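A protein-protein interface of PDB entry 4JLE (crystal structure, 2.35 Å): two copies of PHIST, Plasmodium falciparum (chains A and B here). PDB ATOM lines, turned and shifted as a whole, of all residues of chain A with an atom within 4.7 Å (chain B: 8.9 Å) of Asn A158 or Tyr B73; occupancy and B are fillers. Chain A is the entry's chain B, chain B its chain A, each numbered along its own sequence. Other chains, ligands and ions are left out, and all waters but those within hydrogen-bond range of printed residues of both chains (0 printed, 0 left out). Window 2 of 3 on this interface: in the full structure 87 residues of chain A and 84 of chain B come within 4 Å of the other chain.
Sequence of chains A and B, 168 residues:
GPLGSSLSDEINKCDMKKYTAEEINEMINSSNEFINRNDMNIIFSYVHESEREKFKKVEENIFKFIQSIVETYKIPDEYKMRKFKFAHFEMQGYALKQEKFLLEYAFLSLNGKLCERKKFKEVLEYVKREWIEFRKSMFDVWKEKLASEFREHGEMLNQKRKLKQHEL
Among the printed residues, pairs that only touch across the chains: Arg A151 with Ile B69 (3.6 Å), Arg A151 with Tyr B73 (3.6 Å), Gly A154 with Tyr B73 (3.6 Å), Glu A155 with Tyr B73 (3.9 Å), Leu A157 with Pro B76 (3.8 Å) and Asn A158 with Tyr B73 (3.7 Å).
No position is printed for both chains. Of the 8 pairs that touch across the chains among the printed residues, none has its exchanged pair printed and touching as well.
Printed residues of chain B within 4 Å of Arg A151: Ile B69 (3.6 Å) and Tyr B73 (3.6 Å). Of the printed residues of chain B, Asn A158 touches Tyr B73 (3.7 Å). Arg A161 touches just these residues of chain B: Tyr B73 (2.8 Å) and Lys B74 (2.8 Å). Printed residues of chain A within 4 Å of Ile B69: Arg A151 (3.6 Å). Thr B72 touches none of the printed residues of chain A. Of the printed residues of chain A, Tyr B73 touches Arg A151 (3.6 Å), Gly A154 (3.6 Å), Glu A155 (3.9 Å), Asn A158 (3.7 Å) and Arg A161 (2.8 Å). Of the printed residues of chain A, Lys B74 touches Arg A161 (2.8 Å). Of the printed residues of chain A, Pro B76 touches Leu A157. The nearest residue of chain B that does not touch Asn A158 is Thr B72 (5.6 Å). The nearest printed residue of chain A that does not touch Tyr B73 is Leu A157 (4.7 Å). The nearest printed residue of chain B that does not touch Leu A157 is Ile B75 (4.3 Å).
The side-chain amide oxygen (OD1) of Asn A158 sits at hydrogen-bond distance from the guanidinium group (NH1) of Arg A161.
Printed residues of chain B that touch a printed residue of chain A: Ile B69, Tyr B73, Lys B74 and Pro B76. Among the printed residues, no Asp or Glu carboxylate lies within 4 Å of a Lys or Arg side-chain nitrogen of the other chain.
O of Tyr B73 lies within hydrogen-bond range of NH1 of Arg A161 (2.8 Å). The guanidinium group (NH2) of Arg A161 is in hydrogen-bond range of the backbone carbonyl oxygen (O) of Lys B74 (2.8 Å).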
ATOM      1  N   ARG A 151      -9.993   4.936 -26.436  1.00  0.00           N
ATOM      2  CA  ARG A 151      -9.991   3.662 -27.180  1.00  0.00           C
ATOM      3  C   ARG A 151      -9.715   2.514 -26.212  1.00  0.00           C
ATOM      4  O   ARG A 151     -10.414   1.504 -26.260  1.00  0.00           O
ATOM      5  CB  ARG A 151      -8.961   3.720 -28.325  1.00  0.00           C
ATOM      6  CG  ARG A 151      -9.135   2.713 -29.449  1.00  0.00           C
ATOM      7  CD  ARG A 151      -8.906   3.275 -30.849  1.00  0.00           C
ATOM      8  NE  ARG A 151      -7.750   4.170 -30.981  1.00  0.00           N
ATOM      9  CZ  ARG A 151      -7.751   5.270 -31.731  1.00  0.00           C
ATOM     10  NH1 ARG A 151      -8.846   5.631 -32.389  1.00  0.00           N
ATOM     11  NH2 ARG A 151      -6.667   6.032 -31.805  1.00  0.00           N
ATOM     12  N   GLY A 154     -12.664   2.031 -23.825  1.00  0.00           N
ATOM     13  CA  GLY A 154     -13.717   1.431 -24.635  1.00  0.00           C
ATOM     14  C   GLY A 154     -13.483  -0.048 -24.854  1.00  0.00           C
ATOM     15  O   GLY A 154     -14.438  -0.838 -24.870  1.00  0.00           O
ATOM     16  N   GLU A 155     -12.202  -0.442 -25.017  1.00  0.00           N
ATOM     17  CA  GLU A 155     -11.824  -1.867 -25.169  1.00  0.00           C
ATOM     18  C   GLU A 155     -12.099  -2.623 -23.829  1.00  0.00           C
ATOM     19  O   GLU A 155     -12.696  -3.697 -23.866  1.00  0.00           O
ATOM     20  CB  GLU A 155     -10.372  -2.018 -25.647  1.00  0.00           C
ATOM     21  CG  GLU A 155     -10.190  -1.660 -27.122  1.00  0.00           C
ATOM     22  CD  GLU A 155      -8.792  -1.287 -27.626  1.00  0.00           C
ATOM     23  OE1 GLU A 155      -7.861  -1.105 -26.805  1.00  0.00           O
ATOM     24  OE2 GLU A 155      -8.632  -1.163 -28.862  1.00  0.00           O
ATOM     25  N   MET A 156     -11.747  -2.004 -22.668  1.00  0.00           N
ATOM     26  CA  MET A 156     -11.958  -2.483 -21.292  1.00  0.00           C
ATOM     27  C   MET A 156     -13.454  -2.703 -21.025  1.00  0.00           C
ATOM     28  O   MET A 156     -13.813  -3.695 -20.390  1.00  0.00           O
ATOM     29  CB  MET A 156     -11.349  -1.478 -20.276  1.00  0.00           C
ATOM     30  CG  MET A 156     -11.483  -1.874 -18.801  1.00  0.00           C
ATOM     31  SD  MET A 156     -13.083  -1.406 -18.037  1.00  0.00           S
ATOM     32  CE  MET A 156     -12.683   0.191 -17.361  1.00  0.00           C
ATOM     33  N   LEU A 157     -14.324  -1.775 -21.488  1.00  0.00           N
ATOM     34  CA  LEU A 157     -15.779  -1.895 -21.323  1.00  0.00           C
ATOM     35  C   LEU A 157     -16.317  -3.060 -22.134  1.00  0.00           C
ATOM     36  O   LEU A 157     -17.096  -3.845 -21.605  1.00  0.00           O
ATOM     37  CB  LEU A 157     -16.532  -0.605 -21.711  1.00  0.00           C
ATOM     38  CG  LEU A 157     -16.313   0.648 -20.849  1.00  0.00           C
ATOM     39  CD1 LEU A 157     -17.077   1.824 -21.421  1.00  0.00           C
ATOM     40  CD2 LEU A 157     -16.690   0.420 -19.386  1.00  0.00           C
ATOM     41  N   ASN A 158     -15.907  -3.177 -23.411  1.00  0.00           N
ATOM     42  CA  ASN A 158     -16.346  -4.248 -24.305  1.00  0.00           C
ATOM     43  C   ASN A 158     -15.999  -5.619 -23.692  1.00  0.00           C
ATOM     44  O   ASN A 158     -16.856  -6.513 -23.710  1.00  0.00           O
ATOM     45  CB  ASN A 158     -15.748  -4.068 -25.712  1.00  0.00           C
ATOM     46  CG  ASN A 158     -16.475  -3.068 -26.603  1.00  0.00           C
ATOM     47  OD1 ASN A 158     -17.436  -2.389 -26.202  1.00  0.00           O
ATOM     48  ND2 ASN A 158     -16.040  -2.964 -27.854  1.00  0.00           N
ATOM     49  N   GLN A 159     -14.800  -5.730 -23.042  1.00  0.00           N
ATOM     50  CA  GLN A 159     -14.321  -6.921 -22.315  1.00  0.00           C
ATOM     51  C   GLN A 159     -15.332  -7.320 -21.222  1.00  0.00           C
ATOM     52  O   GLN A 159     -15.853  -8.433 -21.263  1.00  0.00           O
ATOM     53  CB  GLN A 159     -12.933  -6.672 -21.685  1.00  0.00           C
ATOM     54  CG  GLN A 159     -11.760  -6.741 -22.667  1.00  0.00           C
ATOM     55  CD  GLN A 159     -10.486  -6.075 -22.162  1.00  0.00           C
ATOM     56  OE1 GLN A 159     -10.342  -5.705 -20.985  1.00  0.00           O
ATOM     57  NE2 GLN A 159      -9.518  -5.900 -23.051  1.00  0.00           N
ATOM     58  N   LYS A 160     -15.665  -6.375 -20.304  1.00  0.00           N
ATOM     59  CA  LYS A 160     -16.627  -6.572 -19.206  1.00  0.00           C
ATOM     60  C   LYS A 160     -18.031  -6.904 -19.758  1.00  0.00           C
ATOM     61  O   LYS A 160     -18.724  -7.749 -19.178  1.00  0.00           O
ATOM     62  CB  LYS A 160     -16.684  -5.351 -18.268  1.00  0.00           C
ATOM     63  CG  LYS A 160     -15.473  -5.202 -17.379  1.00  0.00           C
ATOM     64  CD  LYS A 160     -15.636  -4.025 -16.439  1.00  0.00           C
ATOM     65  CE  LYS A 160     -14.379  -3.819 -15.620  1.00  0.00           C
ATOM     66  NZ  LYS A 160     -14.270  -2.440 -15.066  1.00  0.00           N
ATOM     67  N   ARG A 161     -18.417  -6.290 -20.906  1.00  0.00           N
ATOM     68  CA  ARG A 161     -19.696  -6.533 -21.586  1.00  0.00           C
ATOM     69  C   ARG A 161     -19.750  -7.950 -22.209  1.00  0.00           C
ATOM     70  O   ARG A 161     -20.776  -8.615 -22.087  1.00  0.00           O
ATOM     71  CB  ARG A 161     -19.960  -5.480 -22.667  1.00  0.00           C
ATOM     72  CG  ARG A 161     -20.366  -4.117 -22.110  1.00  0.00           C
ATOM     73  CD  ARG A 161     -20.061  -3.022 -23.103  1.00  0.00           C
ATOM     74  NE  ARG A 161     -20.352  -1.689 -22.578  1.00  0.00           N
ATOM     75  CZ  ARG A 161     -19.958  -0.561 -23.161  1.00  0.00           C
ATOM     76  NH1 ARG A 161     -19.236  -0.600 -24.275  1.00  0.00           N
ATOM     77  NH2 ARG A 161     -20.269   0.613 -22.626  1.00  0.00           N
ATOM     78  N   LYS A 162     -18.656  -8.396 -22.876  1.00  0.00           N
ATOM     79  CA  LYS A 162     -18.530  -9.723 -23.508  1.00  0.00           C
ATOM     80  C   LYS A 162     -18.590 -10.842 -22.455  1.00  0.00           C
ATOM     81  O   LYS A 162     -19.185 -11.898 -22.708  1.00  0.00           O
ATOM     82  CB  LYS A 162     -17.221  -9.838 -24.319  1.00  0.00           C
ATOM     83  CG  LYS A 162     -17.226  -9.063 -25.634  1.00  0.00           C
ATOM     84  CD  LYS A 162     -15.950  -9.296 -26.447  1.00  0.00           C
ATOM     85  CE  LYS A 162     -14.794  -8.420 -26.008  1.00  0.00           C
ATOM     86  NZ  LYS A 162     -13.599  -8.614 -26.864  1.00  0.00           N
ATOM     87  N   ILE B  66     -12.930  12.859 -30.592  1.00  0.00           N
ATOM     88  CA  ILE B  66     -13.050  11.869 -29.519  1.00  0.00           C
ATOM     89  C   ILE B  66     -14.520  11.378 -29.422  1.00  0.00           C
ATOM     90  O   ILE B  66     -14.751  10.234 -29.032  1.00  0.00           O
ATOM     91  CB  ILE B  66     -12.473  12.410 -28.161  1.00  0.00           C
ATOM     92  CG1 ILE B  66     -10.994  12.875 -28.299  1.00  0.00           C
ATOM     93  CG2 ILE B  66     -12.614  11.393 -27.019  1.00  0.00           C
ATOM     94  CD1 ILE B  66      -9.975  11.855 -28.848  1.00  0.00           C
ATOM     95  N   GLN B  67     -15.485  12.191 -29.871  1.00  0.00           N
ATOM     96  CA  GLN B  67     -16.897  11.829 -29.895  1.00  0.00           C
ATOM     97  C   GLN B  67     -17.126  10.602 -30.780  1.00  0.00           C
ATOM     98  O   GLN B  67     -17.922   9.745 -30.410  1.00  0.00           O
ATOM     99  CB  GLN B  67     -17.765  13.017 -30.343  1.00  0.00           C
ATOM    100  CG  GLN B  67     -19.290  12.788 -30.246  1.00  0.00           C
ATOM    101  CD  GLN B  67     -19.756  12.375 -28.873  1.00  0.00           C
ATOM    102  OE1 GLN B  67     -19.253  12.846 -27.862  1.00  0.00           O
ATOM    103  NE2 GLN B  67     -20.733  11.482 -28.807  1.00  0.00           N
ATOM    104  N   SER B  68     -16.346  10.466 -31.880  1.00  0.00           N
ATOM    105  CA  SER B  68     -16.398   9.326 -32.802  1.00  0.00           C
ATOM    106  C   SER B  68     -16.010   8.026 -32.111  1.00  0.00           C
ATOM    107  O   SER B  68     -16.586   6.982 -32.420  1.00  0.00           O
ATOM    108  CB  SER B  68     -15.513   9.575 -34.012  1.00  0.00           C
ATOM    109  OG  SER B  68     -14.138   9.439 -33.705  1.00  0.00           O
ATOM    110  N   ILE B  69     -15.034   8.077 -31.184  1.00  0.00           N
ATOM    111  CA  ILE B  69     -14.541   6.916 -30.406  1.00  0.00           C
ATOM    112  C   ILE B  69     -15.565   6.610 -29.313  1.00  0.00           C
ATOM    113  O   ILE B  69     -15.823   5.442 -29.026  1.00  0.00           O
ATOM    114  CB  ILE B  69     -13.110   7.196 -29.817  1.00  0.00           C
ATOM    115  CG1 ILE B  69     -12.111   7.546 -30.951  1.00  0.00           C
ATOM    116  CG2 ILE B  69     -12.598   5.997 -28.950  1.00  0.00           C
ATOM    117  CD1 ILE B  69     -10.768   8.078 -30.491  1.00  0.00           C
ATOM    118  N   VAL B  70     -16.175   7.678 -28.730  1.00  0.00           N
ATOM    119  CA  VAL B  70     -17.195   7.567 -27.689  1.00  0.00           C
ATOM    120  C   VAL B  70     -18.376   6.738 -28.209  1.00  0.00           C
ATOM    121  O   VAL B  70     -18.804   5.803 -27.532  1.00  0.00           O
ATOM    122  CB  VAL B  70     -17.635   8.961 -27.158  1.00  0.00           C
ATOM    123  CG1 VAL B  70     -18.932   8.866 -26.361  1.00  0.00           C
ATOM    124  CG2 VAL B  70     -16.531   9.591 -26.323  1.00  0.00           C
ATOM    125  N   GLU B  71     -18.846   7.059 -29.430  1.00  0.00           N
ATOM    126  CA  GLU B  71     -19.953   6.394 -30.109  1.00  0.00           C
ATOM    127  C   GLU B  71     -19.567   4.986 -30.588  1.00  0.00           C
ATOM    128  O   GLU B  71     -20.381   4.082 -30.483  1.00  0.00           O
ATOM    129  CB  GLU B  71     -20.448   7.258 -31.277  1.00  0.00           C
ATOM    130  CG  GLU B  71     -21.073   8.564 -30.785  1.00  0.00           C
ATOM    131  CD  GLU B  71     -21.906   9.370 -31.753  1.00  0.00           C
ATOM    132  OE1 GLU B  71     -22.628   8.757 -32.574  1.00  0.00           O
ATOM    133  OE2 GLU B  71     -21.932  10.613 -31.604  1.00  0.00           O
ATOM    134  N   THR B  72     -18.317   4.782 -31.053  1.00  0.00           N
ATOM    135  CA  THR B  72     -17.849   3.464 -31.476  1.00  0.00           C
ATOM    136  C   THR B  72     -17.886   2.468 -30.294  1.00  0.00           C
ATOM    137  O   THR B  72     -18.368   1.357 -30.458  1.00  0.00           O
ATOM    138  CB  THR B  72     -16.436   3.561 -32.092  1.00  0.00           C
ATOM    139  OG1 THR B  72     -16.506   4.372 -33.268  1.00  0.00           O
ATOM    140  CG2 THR B  72     -15.825   2.195 -32.427  1.00  0.00           C
ATOM    141  N   TYR B  73     -17.418   2.883 -29.115  1.00  0.00           N
ATOM    142  CA  TYR B  73     -17.347   2.011 -27.952  1.00  0.00           C
ATOM    143  C   TYR B  73     -18.486   2.210 -26.959  1.00  0.00           C
ATOM    144  O   TYR B  73     -18.456   1.583 -25.895  1.00  0.00           O
ATOM    145  CB  TYR B  73     -15.994   2.218 -27.251  1.00  0.00           C
ATOM    146  CG  TYR B  73     -14.840   1.743 -28.097  1.00  0.00           C
ATOM    147  CD1 TYR B  73     -14.551   0.387 -28.219  1.00  0.00           C
ATOM    148  CD2 TYR B  73     -14.082   2.642 -28.839  1.00  0.00           C
ATOM    149  CE1 TYR B  73     -13.504  -0.059 -29.020  1.00  0.00           C
ATOM    150  CE2 TYR B  73     -13.034   2.208 -29.645  1.00  0.00           C
ATOM    151  CZ  TYR B  73     -12.747   0.856 -29.733  1.00  0.00           C
ATOM    152  OH  TYR B  73     -11.713   0.423 -30.541  1.00  0.00           O
ATOM    153  N   LYS B  74     -19.489   3.073 -27.286  1.00  0.00           N
ATOM    154  CA  LYS B  74     -20.631   3.351 -26.417  1.00  0.00           C
ATOM    155  C   LYS B  74     -20.111   3.711 -24.995  1.00  0.00           C
ATOM    156  O   LYS B  74     -20.470   3.079 -23.993  1.00  0.00           O
ATOM    157  CB  LYS B  74     -21.635   2.162 -26.396  1.00  0.00           C
ATOM    158  CG  LYS B  74     -22.278   1.856 -27.741  1.00  0.00           C
ATOM    159  CD  LYS B  74     -23.032   0.549 -27.652  1.00  0.00           C
ATOM    160  CE  LYS B  74     -23.555   0.073 -28.981  1.00  0.00           C
ATOM    161  NZ  LYS B  74     -24.301  -1.208 -28.843  1.00  0.00           N
ATOM    162  N   ILE B  75     -19.192   4.686 -24.938  1.00  0.00           N
ATOM    163  CA  ILE B  75     -18.603   5.154 -23.692  1.00  0.00           C
ATOM    164  C   ILE B  75     -19.636   6.061 -22.980  1.00  0.00           C
ATOM    165  O   ILE B  75     -20.190   6.956 -23.625  1.00  0.00           O
ATOM    166  CB  ILE B  75     -17.246   5.851 -23.960  1.00  0.00           C
ATOM    167  CG1 ILE B  75     -16.186   4.796 -24.404  1.00  0.00           C
ATOM    168  CG2 ILE B  75     -16.768   6.698 -22.747  1.00  0.00           C
ATOM    169  CD1 ILE B  75     -14.968   5.356 -25.081  1.00  0.00           C
ATOM    170  N   PRO B  76     -19.945   5.829 -21.677  1.00  0.00           N
ATOM    171  CA  PRO B  76     -20.958   6.690 -21.002  1.00  0.00           C
ATOM    172  C   PRO B  76     -20.485   8.132 -20.869  1.00  0.00           C
ATOM    173  O   PRO B  76     -19.297   8.385 -20.760  1.00  0.00           O
ATOM    174  CB  PRO B  76     -21.160   6.030 -19.630  1.00  0.00           C
ATOM    175  CG  PRO B  76     -20.564   4.615 -19.780  1.00  0.00           C
ATOM    176  CD  PRO B  76     -19.422   4.792 -20.758  1.00  0.00           C
